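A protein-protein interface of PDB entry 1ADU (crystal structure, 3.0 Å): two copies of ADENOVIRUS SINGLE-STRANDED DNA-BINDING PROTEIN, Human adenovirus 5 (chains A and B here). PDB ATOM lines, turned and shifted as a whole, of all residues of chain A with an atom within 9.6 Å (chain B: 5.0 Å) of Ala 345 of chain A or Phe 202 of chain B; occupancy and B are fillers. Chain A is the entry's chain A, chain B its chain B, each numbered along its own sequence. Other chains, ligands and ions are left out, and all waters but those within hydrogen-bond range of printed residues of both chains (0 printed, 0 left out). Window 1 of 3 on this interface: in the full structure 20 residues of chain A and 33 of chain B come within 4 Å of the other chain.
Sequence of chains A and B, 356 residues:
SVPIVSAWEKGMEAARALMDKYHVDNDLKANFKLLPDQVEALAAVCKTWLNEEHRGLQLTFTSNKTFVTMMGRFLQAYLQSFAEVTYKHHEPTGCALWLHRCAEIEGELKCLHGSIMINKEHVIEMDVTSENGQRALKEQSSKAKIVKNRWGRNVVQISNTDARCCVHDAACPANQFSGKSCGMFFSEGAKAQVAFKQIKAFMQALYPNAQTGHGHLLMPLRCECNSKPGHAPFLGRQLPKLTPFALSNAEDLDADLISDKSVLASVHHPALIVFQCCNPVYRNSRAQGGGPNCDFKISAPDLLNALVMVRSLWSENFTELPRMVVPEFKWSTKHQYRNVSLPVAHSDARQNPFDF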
ATOM      1  N   LEU A 342      31.109 -16.683 -19.287  1.00  0.00           N
ATOM      2  CA  LEU A 342      30.794 -16.241 -17.938  1.00  0.00           C
ATOM      3  C   LEU A 342      30.023 -14.933 -18.110  1.00  0.00           C
ATOM      4  O   LEU A 342      30.358 -14.114 -18.974  1.00  0.00           O
ATOM      5  CB  LEU A 342      32.071 -16.016 -17.124  1.00  0.00           C
ATOM      6  CG  LEU A 342      33.019 -17.206 -16.925  1.00  0.00           C
ATOM      7  CD1 LEU A 342      34.119 -16.818 -15.939  1.00  0.00           C
ATOM      8  CD2 LEU A 342      32.254 -18.423 -16.420  1.00  0.00           C
ATOM      9  N   PRO A 343      28.956 -14.738 -17.321  1.00  0.00           N
ATOM     10  CA  PRO A 343      28.137 -13.527 -17.402  1.00  0.00           C
ATOM     11  C   PRO A 343      28.874 -12.232 -17.079  1.00  0.00           C
ATOM     12  O   PRO A 343      29.485 -12.099 -16.012  1.00  0.00           O
ATOM     13  CB  PRO A 343      27.035 -13.794 -16.376  1.00  0.00           C
ATOM     14  CG  PRO A 343      26.937 -15.284 -16.362  1.00  0.00           C
ATOM     15  CD  PRO A 343      28.379 -15.686 -16.354  1.00  0.00           C
ATOM     16  N   VAL A 344      28.823 -11.291 -18.017  1.00  0.00           N
ATOM     17  CA  VAL A 344      29.432  -9.976 -17.836  1.00  0.00           C
ATOM     18  C   VAL A 344      28.298  -8.962 -17.801  1.00  0.00           C
ATOM     19  O   VAL A 344      27.365  -9.025 -18.607  1.00  0.00           O
ATOM     20  CB  VAL A 344      30.414  -9.606 -18.970  1.00  0.00           C
ATOM     21  CG1 VAL A 344      31.692 -10.408 -18.839  1.00  0.00           C
ATOM     22  CG2 VAL A 344      29.777  -9.847 -20.330  1.00  0.00           C
ATOM     23  N   ALA A 345      28.361  -8.059 -16.833  1.00  0.00           N
ATOM     24  CA  ALA A 345      27.343  -7.032 -16.659  1.00  0.00           C
ATOM     25  C   ALA A 345      27.227  -6.060 -17.833  1.00  0.00           C
ATOM     26  O   ALA A 345      27.860  -6.236 -18.876  1.00  0.00           O
ATOM     27  CB  ALA A 345      27.613  -6.262 -15.377  1.00  0.00           C
ATOM     28  N   HIS A 346      26.374  -5.056 -17.678  1.00  0.00           N
ATOM     29  CA  HIS A 346      26.166  -4.031 -18.692  1.00  0.00           C
ATOM     30  C   HIS A 346      25.932  -2.716 -17.969  1.00  0.00           C
ATOM     31  O   HIS A 346      25.139  -2.650 -17.030  1.00  0.00           O
ATOM     32  CB  HIS A 346      24.970  -4.369 -19.582  1.00  0.00           C
ATOM     33  CG  HIS A 346      25.308  -5.262 -20.735  1.00  0.00           C
ATOM     34  ND1 HIS A 346      25.948  -6.474 -20.582  1.00  0.00           N
ATOM     35  CD2 HIS A 346      25.098  -5.117 -22.065  1.00  0.00           C
ATOM     36  CE1 HIS A 346      26.116  -7.037 -21.763  1.00  0.00           C
ATOM     37  NE2 HIS A 346      25.608  -6.234 -22.681  1.00  0.00           N
ATOM     38  N   SER A 347      26.656  -1.686 -18.393  1.00  0.00           N
ATOM     39  CA  SER A 347      26.575  -0.362 -17.787  1.00  0.00           C
ATOM     40  C   SER A 347      25.173   0.232 -17.711  1.00  0.00           C
ATOM     41  O   SER A 347      24.546   0.517 -18.733  1.00  0.00           O
ATOM     42  CB  SER A 347      27.512   0.603 -18.514  1.00  0.00           C
ATOM     43  OG  SER A 347      28.843   0.111 -18.501  1.00  0.00           O
ATOM     44  N   ASP A 348      24.695   0.416 -16.487  1.00  0.00           N
ATOM     45  CA  ASP A 348      23.382   0.989 -16.246  1.00  0.00           C
ATOM     46  C   ASP A 348      23.585   2.248 -15.408  1.00  0.00           C
ATOM     47  O   ASP A 348      24.109   2.185 -14.294  1.00  0.00           O
ATOM     48  CB  ASP A 348      22.497  -0.009 -15.490  1.00  0.00           C
ATOM     49  CG  ASP A 348      21.025   0.396 -15.473  1.00  0.00           C
ATOM     50  OD1 ASP A 348      20.716   1.608 -15.470  1.00  0.00           O
ATOM     51  OD2 ASP A 348      20.167  -0.512 -15.462  1.00  0.00           O
ATOM     52  N   PRO A 353      18.718  -0.739  -8.790  1.00  0.00           N
ATOM     53  CA  PRO A 353      18.381  -1.673  -9.872  1.00  0.00           C
ATOM     54  C   PRO A 353      16.901  -1.774 -10.240  1.00  0.00           C
ATOM     55  O   PRO A 353      16.568  -1.971 -11.409  1.00  0.00           O
ATOM     56  CB  PRO A 353      18.913  -3.007  -9.346  1.00  0.00           C
ATOM     57  CG  PRO A 353      18.783  -2.871  -7.873  1.00  0.00           C
ATOM     58  CD  PRO A 353      19.248  -1.461  -7.621  1.00  0.00           C
ATOM     59  N   GLN B 198      25.845 -16.139  -6.059  1.00  0.00           N
ATOM     60  CA  GLN B 198      26.416 -15.600  -7.293  1.00  0.00           C
ATOM     61  C   GLN B 198      25.607 -14.417  -7.799  1.00  0.00           C
ATOM     62  O   GLN B 198      26.159 -13.348  -8.044  1.00  0.00           O
ATOM     63  CB  GLN B 198      26.497 -16.694  -8.369  1.00  0.00           C
ATOM     64  CG  GLN B 198      27.124 -16.261  -9.704  1.00  0.00           C
ATOM     65  CD  GLN B 198      26.128 -15.604 -10.647  1.00  0.00           C
ATOM     66  OE1 GLN B 198      26.228 -14.419 -10.952  1.00  0.00           O
ATOM     67  NE2 GLN B 198      25.142 -16.366 -11.083  1.00  0.00           N
ATOM     68  N   ILE B 199      24.296 -14.604  -7.927  1.00  0.00           N
ATOM     69  CA  ILE B 199      23.431 -13.537  -8.413  1.00  0.00           C
ATOM     70  C   ILE B 199      23.463 -12.341  -7.470  1.00  0.00           C
ATOM     71  O   ILE B 199      23.462 -11.194  -7.921  1.00  0.00           O
ATOM     72  CB  ILE B 199      21.974 -14.022  -8.655  1.00  0.00           C
ATOM     73  CG1 ILE B 199      21.208 -12.981  -9.475  1.00  0.00           C
ATOM     74  CG2 ILE B 199      21.259 -14.275  -7.342  1.00  0.00           C
ATOM     75  CD1 ILE B 199      21.854 -12.645 -10.813  1.00  0.00           C
ATOM     76  N   LYS B 200      23.547 -12.604  -6.169  1.00  0.00           N
ATOM     77  CA  LYS B 200      23.602 -11.523  -5.190  1.00  0.00           C
ATOM     78  C   LYS B 200      24.876 -10.719  -5.443  1.00  0.00           C
ATOM     79  O   LYS B 200      24.880  -9.489  -5.355  1.00  0.00           O
ATOM     80  CB  LYS B 200      23.590 -12.076  -3.756  1.00  0.00           C
ATOM     81  CG  LYS B 200      23.434 -11.007  -2.675  1.00  0.00           C
ATOM     82  CD  LYS B 200      23.477 -11.619  -1.284  1.00  0.00           C
ATOM     83  CE  LYS B 200      23.204 -10.586  -0.199  1.00  0.00           C
ATOM     84  NZ  LYS B 200      24.223  -9.499  -0.150  1.00  0.00           N
ATOM     85  N   ALA B 201      25.944 -11.419  -5.810  1.00  0.00           N
ATOM     86  CA  ALA B 201      27.223 -10.788  -6.091  1.00  0.00           C
ATOM     87  C   ALA B 201      27.129  -9.986  -7.380  1.00  0.00           C
ATOM     88  O   ALA B 201      27.420  -8.788  -7.395  1.00  0.00           O
ATOM     89  CB  ALA B 201      28.319 -11.838  -6.202  1.00  0.00           C
ATOM     90  N   PHE B 202      26.686 -10.641  -8.447  1.00  0.00           N
ATOM     91  CA  PHE B 202      26.544 -10.008  -9.754  1.00  0.00           C
ATOM     92  C   PHE B 202      25.811  -8.672  -9.642  1.00  0.00           C
ATOM     93  O   PHE B 202      26.284  -7.652 -10.152  1.00  0.00           O
ATOM     94  CB  PHE B 202      25.785 -10.946 -10.695  1.00  0.00           C
ATOM     95  CG  PHE B 202      25.777 -10.510 -12.142  1.00  0.00           C
ATOM     96  CD1 PHE B 202      26.870 -10.752 -12.961  1.00  0.00           C
ATOM     97  CD2 PHE B 202      24.642  -9.932 -12.705  1.00  0.00           C
ATOM     98  CE1 PHE B 202      26.827 -10.426 -14.315  1.00  0.00           C
ATOM     99  CE2 PHE B 202      24.595  -9.605 -14.061  1.00  0.00           C
ATOM    100  CZ  PHE B 202      25.687  -9.856 -14.863  1.00  0.00           C
ATOM    101  N   MET B 203      24.688  -8.665  -8.930  1.00  0.00           N
ATOM    102  CA  MET B 203      23.896  -7.450  -8.767  1.00  0.00           C
ATOM    103  C   MET B 203      24.594  -6.324  -8.022  1.00  0.00           C
ATOM    104  O   MET B 203      24.270  -5.153  -8.224  1.00  0.00           O
ATOM    105  CB  MET B 203      22.555  -7.759  -8.111  1.00  0.00           C
ATOM    106  CG  MET B 203      21.579  -8.438  -9.041  1.00  0.00           C
ATOM    107  SD  MET B 203      19.942  -8.491  -8.348  1.00  0.00           S
ATOM    108  CE  MET B 203      19.483  -6.794  -8.469  1.00  0.00           C
ATOM    109  N   GLN B 204      25.522  -6.673  -7.135  1.00  0.00           N
ATOM    110  CA  GLN B 204      26.267  -5.667  -6.379  1.00  0.00           C
ATOM    111  C   GLN B 204      27.385  -5.096  -7.244  1.00  0.00           C
ATOM    112  O   GLN B 204      27.754  -3.933  -7.106  1.00  0.00           O
ATOM    113  CB  GLN B 204      26.863  -6.265  -5.109  1.00  0.00           C
ATOM    114  CG  GLN B 204      25.841  -6.912  -4.216  1.00  0.00           C
ATOM    115  CD  GLN B 204      26.280  -6.956  -2.777  1.00  0.00           C
ATOM    116  OE1 GLN B 204      25.848  -6.135  -1.968  1.00  0.00           O
ATOM    117  NE2 GLN B 204      27.139  -7.910  -2.443  1.00  0.00           N
ATOM    118  N   ALA B 205      27.933  -5.935  -8.120  1.00  0.00           N
ATOM    119  CA  ALA B 205      28.999  -5.520  -9.024  1.00  0.00           C
ATOM    120  C   ALA B 205      28.411  -4.532 -10.016  1.00  0.00           C
ATOM    121  O   ALA B 205      28.996  -3.485 -10.293  1.00  0.00           O
ATOM    122  CB  ALA B 205      29.569  -6.722  -9.759  1.00  0.00           C
ATOM    123  N   LEU B 206      27.244  -4.883 -10.547  1.00  0.00           N
ATOM    124  CA  LEU B 206      26.543  -4.044 -11.508  1.00  0.00           C
ATOM    125  C   LEU B 206      26.025  -2.762 -10.823  1.00  0.00           C
ATOM    126  O   LEU B 206      26.163  -1.666 -11.363  1.00  0.00           O
ATOM    127  CB  LEU B 206      25.386  -4.839 -12.124  1.00  0.00           C
ATOM    128  CG  LEU B 206      24.998  -4.607 -13.586  1.00  0.00           C
ATOM    129  CD1 LEU B 206      24.060  -5.710 -14.025  1.00  0.00           C
ATOM    130  CD2 LEU B 206      24.361  -3.244 -13.790  1.00  0.00           C
ATOM    131  N   TYR B 207      25.438  -2.907  -9.636  1.00  0.00           N
ATOM    132  CA  TYR B 207      24.904  -1.772  -8.876  1.00  0.00           C
ATOM    133  C   TYR B 207      25.666  -1.669  -7.557  1.00  0.00           C
ATOM    134  O   TYR B 207      25.235  -2.220  -6.540  1.00  0.00           O
ATOM    135  CB  TYR B 207      23.405  -1.967  -8.600  1.00  0.00           C
ATOM    136  CG  TYR B 207      22.564  -2.078  -9.850  1.00  0.00           C
ATOM    137  CD1 TYR B 207      22.077  -0.936 -10.490  1.00  0.00           C
ATOM    138  CD2 TYR B 207      22.300  -3.320 -10.426  1.00  0.00           C
ATOM    139  CE1 TYR B 207      21.358  -1.025 -11.673  1.00  0.00           C
ATOM    140  CE2 TYR B 207      21.582  -3.424 -11.611  1.00  0.00           C
ATOM    141  CZ  TYR B 207      21.115  -2.273 -12.231  1.00  0.00           C
ATOM    142  OH  TYR B 207      20.404  -2.377 -13.407  1.00  0.00           O
ATOM    143  N   SER B 262      31.986  -8.163 -11.858  1.00  0.00           N
ATOM    144  CA  SER B 262      30.842  -8.976 -12.248  1.00  0.00           C
ATOM    145  C   SER B 262      31.333 -10.389 -12.588  1.00  0.00           C
ATOM    146  O   SER B 262      30.697 -11.388 -12.234  1.00  0.00           O
ATOM    147  CB  SER B 262      30.126  -8.346 -13.445  1.00  0.00           C
ATOM    148  OG  SER B 262      31.000  -8.173 -14.550  1.00  0.00           O
ATOM    149  N   ALA B 265      32.195 -12.444  -9.635  1.00  0.00           N
ATOM    150  CA  ALA B 265      31.059 -13.068  -8.957  1.00  0.00           C
ATOM    151  C   ALA B 265      30.963 -14.530  -9.371  1.00  0.00           C
ATOM    152  O   ALA B 265      30.856 -15.418  -8.525  1.00  0.00           O
ATOM    153  CB  ALA B 265      29.770 -12.343  -9.301  1.00  0.00           C
ATOM    154  N   PRO B 301      21.405 -13.787 -14.548  1.00  0.00           N
ATOM    155  CA  PRO B 301      22.121 -12.581 -14.985  1.00  0.00           C
ATOM    156  C   PRO B 301      21.742 -12.101 -16.384  1.00  0.00           C
ATOM    157  O   PRO B 301      21.666 -10.898 -16.623  1.00  0.00           O
ATOM    158  CB  PRO B 301      23.589 -13.005 -14.887  1.00  0.00           C
ATOM    159  CG  PRO B 301      23.533 -14.481 -15.116  1.00  0.00           C
ATOM    160  CD  PRO B 301      22.355 -14.886 -14.293  1.00  0.00           C
ATOM    161  N   LEU B 304      18.607 -10.102 -16.217  1.00  0.00           N
ATOM    162  CA  LEU B 304      18.896  -8.777 -15.682  1.00  0.00           C
ATOM    163  C   LEU B 304      19.490  -7.909 -16.797  1.00  0.00           C
ATOM    164  O   LEU B 304      19.138  -6.735 -16.928  1.00  0.00           O
ATOM    165  CB  LEU B 304      19.864  -8.883 -14.498  1.00  0.00           C
ATOM    166  CG  LEU B 304      20.198  -7.604 -13.735  1.00  0.00           C
ATOM    167  CD1 LEU B 304      18.936  -6.940 -13.224  1.00  0.00           C
ATOM    168  CD2 LEU B 304      21.116  -7.947 -12.575  1.00  0.00           C
ATOM    169  N   ASN B 305      20.356  -8.499 -17.624  1.00  0.00           N
ATOM    170  CA  ASN B 305      20.963  -7.773 -18.742  1.00  0.00           C
ATOM    171  C   ASN B 305      19.869  -7.382 -19.727  1.00  0.00           C
ATOM    172  O   ASN B 305      19.895  -6.286 -20.282  1.00  0.00           O
ATOM    173  CB  ASN B 305      22.025  -8.614 -19.465  1.00  0.00           C
ATOM    174  CG  ASN B 305      23.399  -8.515 -18.821  1.00  0.00           C
ATOM    175  OD1 ASN B 305      23.726  -7.534 -18.153  1.00  0.00           O
ATOM    176  ND2 ASN B 305      24.226  -9.524 -19.051  1.00  0.00           N
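Phe 202 of chain B touches Pro 343 of chain A.
Pro 343 of chain A touches Pro 301 of chain B (CG to CG, 3.7 Å).
Phe 202 of chain B touches Ala 345 of chain A.
CB of Ala 345 of chain A touches CG of Leu 206 of chain B, at 3.6 Å.
Ala 345 of chain A touches Asn 305 of chain B (C to OD1, 3.8 Å).
Leu 206 of chain B touches His 346 of chain A.
CE of Met 203 of chain B touches CB of Pro 353 of chain A (3.9 Å).
Pro 353 of chain A touches Tyr 207 of chain B.
Printed residues of chain B that touch a printed residue of chain A: Phe 202, Met 203, Leu 206, Tyr 207, Ser 262, Pro 301 and Asn 305.
Among the printed residues, no Asp or Glu carboxylate lies within 4 Å of a Lys or Arg side-chain nitrogen of the other chain.
No position is printed for both chains.
The side-chain hydroxyl (OH) of Tyr 207 of chain B sits at hydrogen-bond distance from the side-chain carboxylate (OD2) of Asp 348 of chain A (2.8 Å).
The backbone carbonyl oxygen of Val 344 of chain A is in hydrogen-bond range of the side-chain amide nitrogen of Asn 305 of chain B (3.2 Å).
The side-chain hydroxyl of Ser 262 of chain B sits at hydrogen-bond distance from the backbone NH of Ala 345 of chain A, at 3.5 Å.
ND1 of His 346 of chain A is in hydrogen-bond range of OD1 of Asn 305 of chain B (3.5 Å).
Ala 345 of chain A touches just these residues of chain B: Phe 202 (3.7 Å), Leu 206 (3.6 Å), Ser 262 (3.5 Å) and Asn 305 (3.8 Å).
Phe 202 of chain B touches two residues of chain A.
Ala 201 of chain B touches none of the printed residues of chain A.
No residue of chain A comes within 4 Å of Ala 205 of chain B.
Printed residues of chain A within 4 Å of Pro 301 of chain B: Pro 343 (3.7 Å).
Of the printed residues of chain B, Asp 348 of chain A touches Tyr 207.
Of the printed residues of chain B, Pro 353 of chain A touches Met 203 and Tyr 207.
Leu 304 of chain B touches none of the printed residues of chain A.
Ile 199 of chain B touches none of the printed residues of chain A.
The nearest printed residue of chain B that does not touch Ala 345 of chain A is Ala 205 of chain B (5.7 Å).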
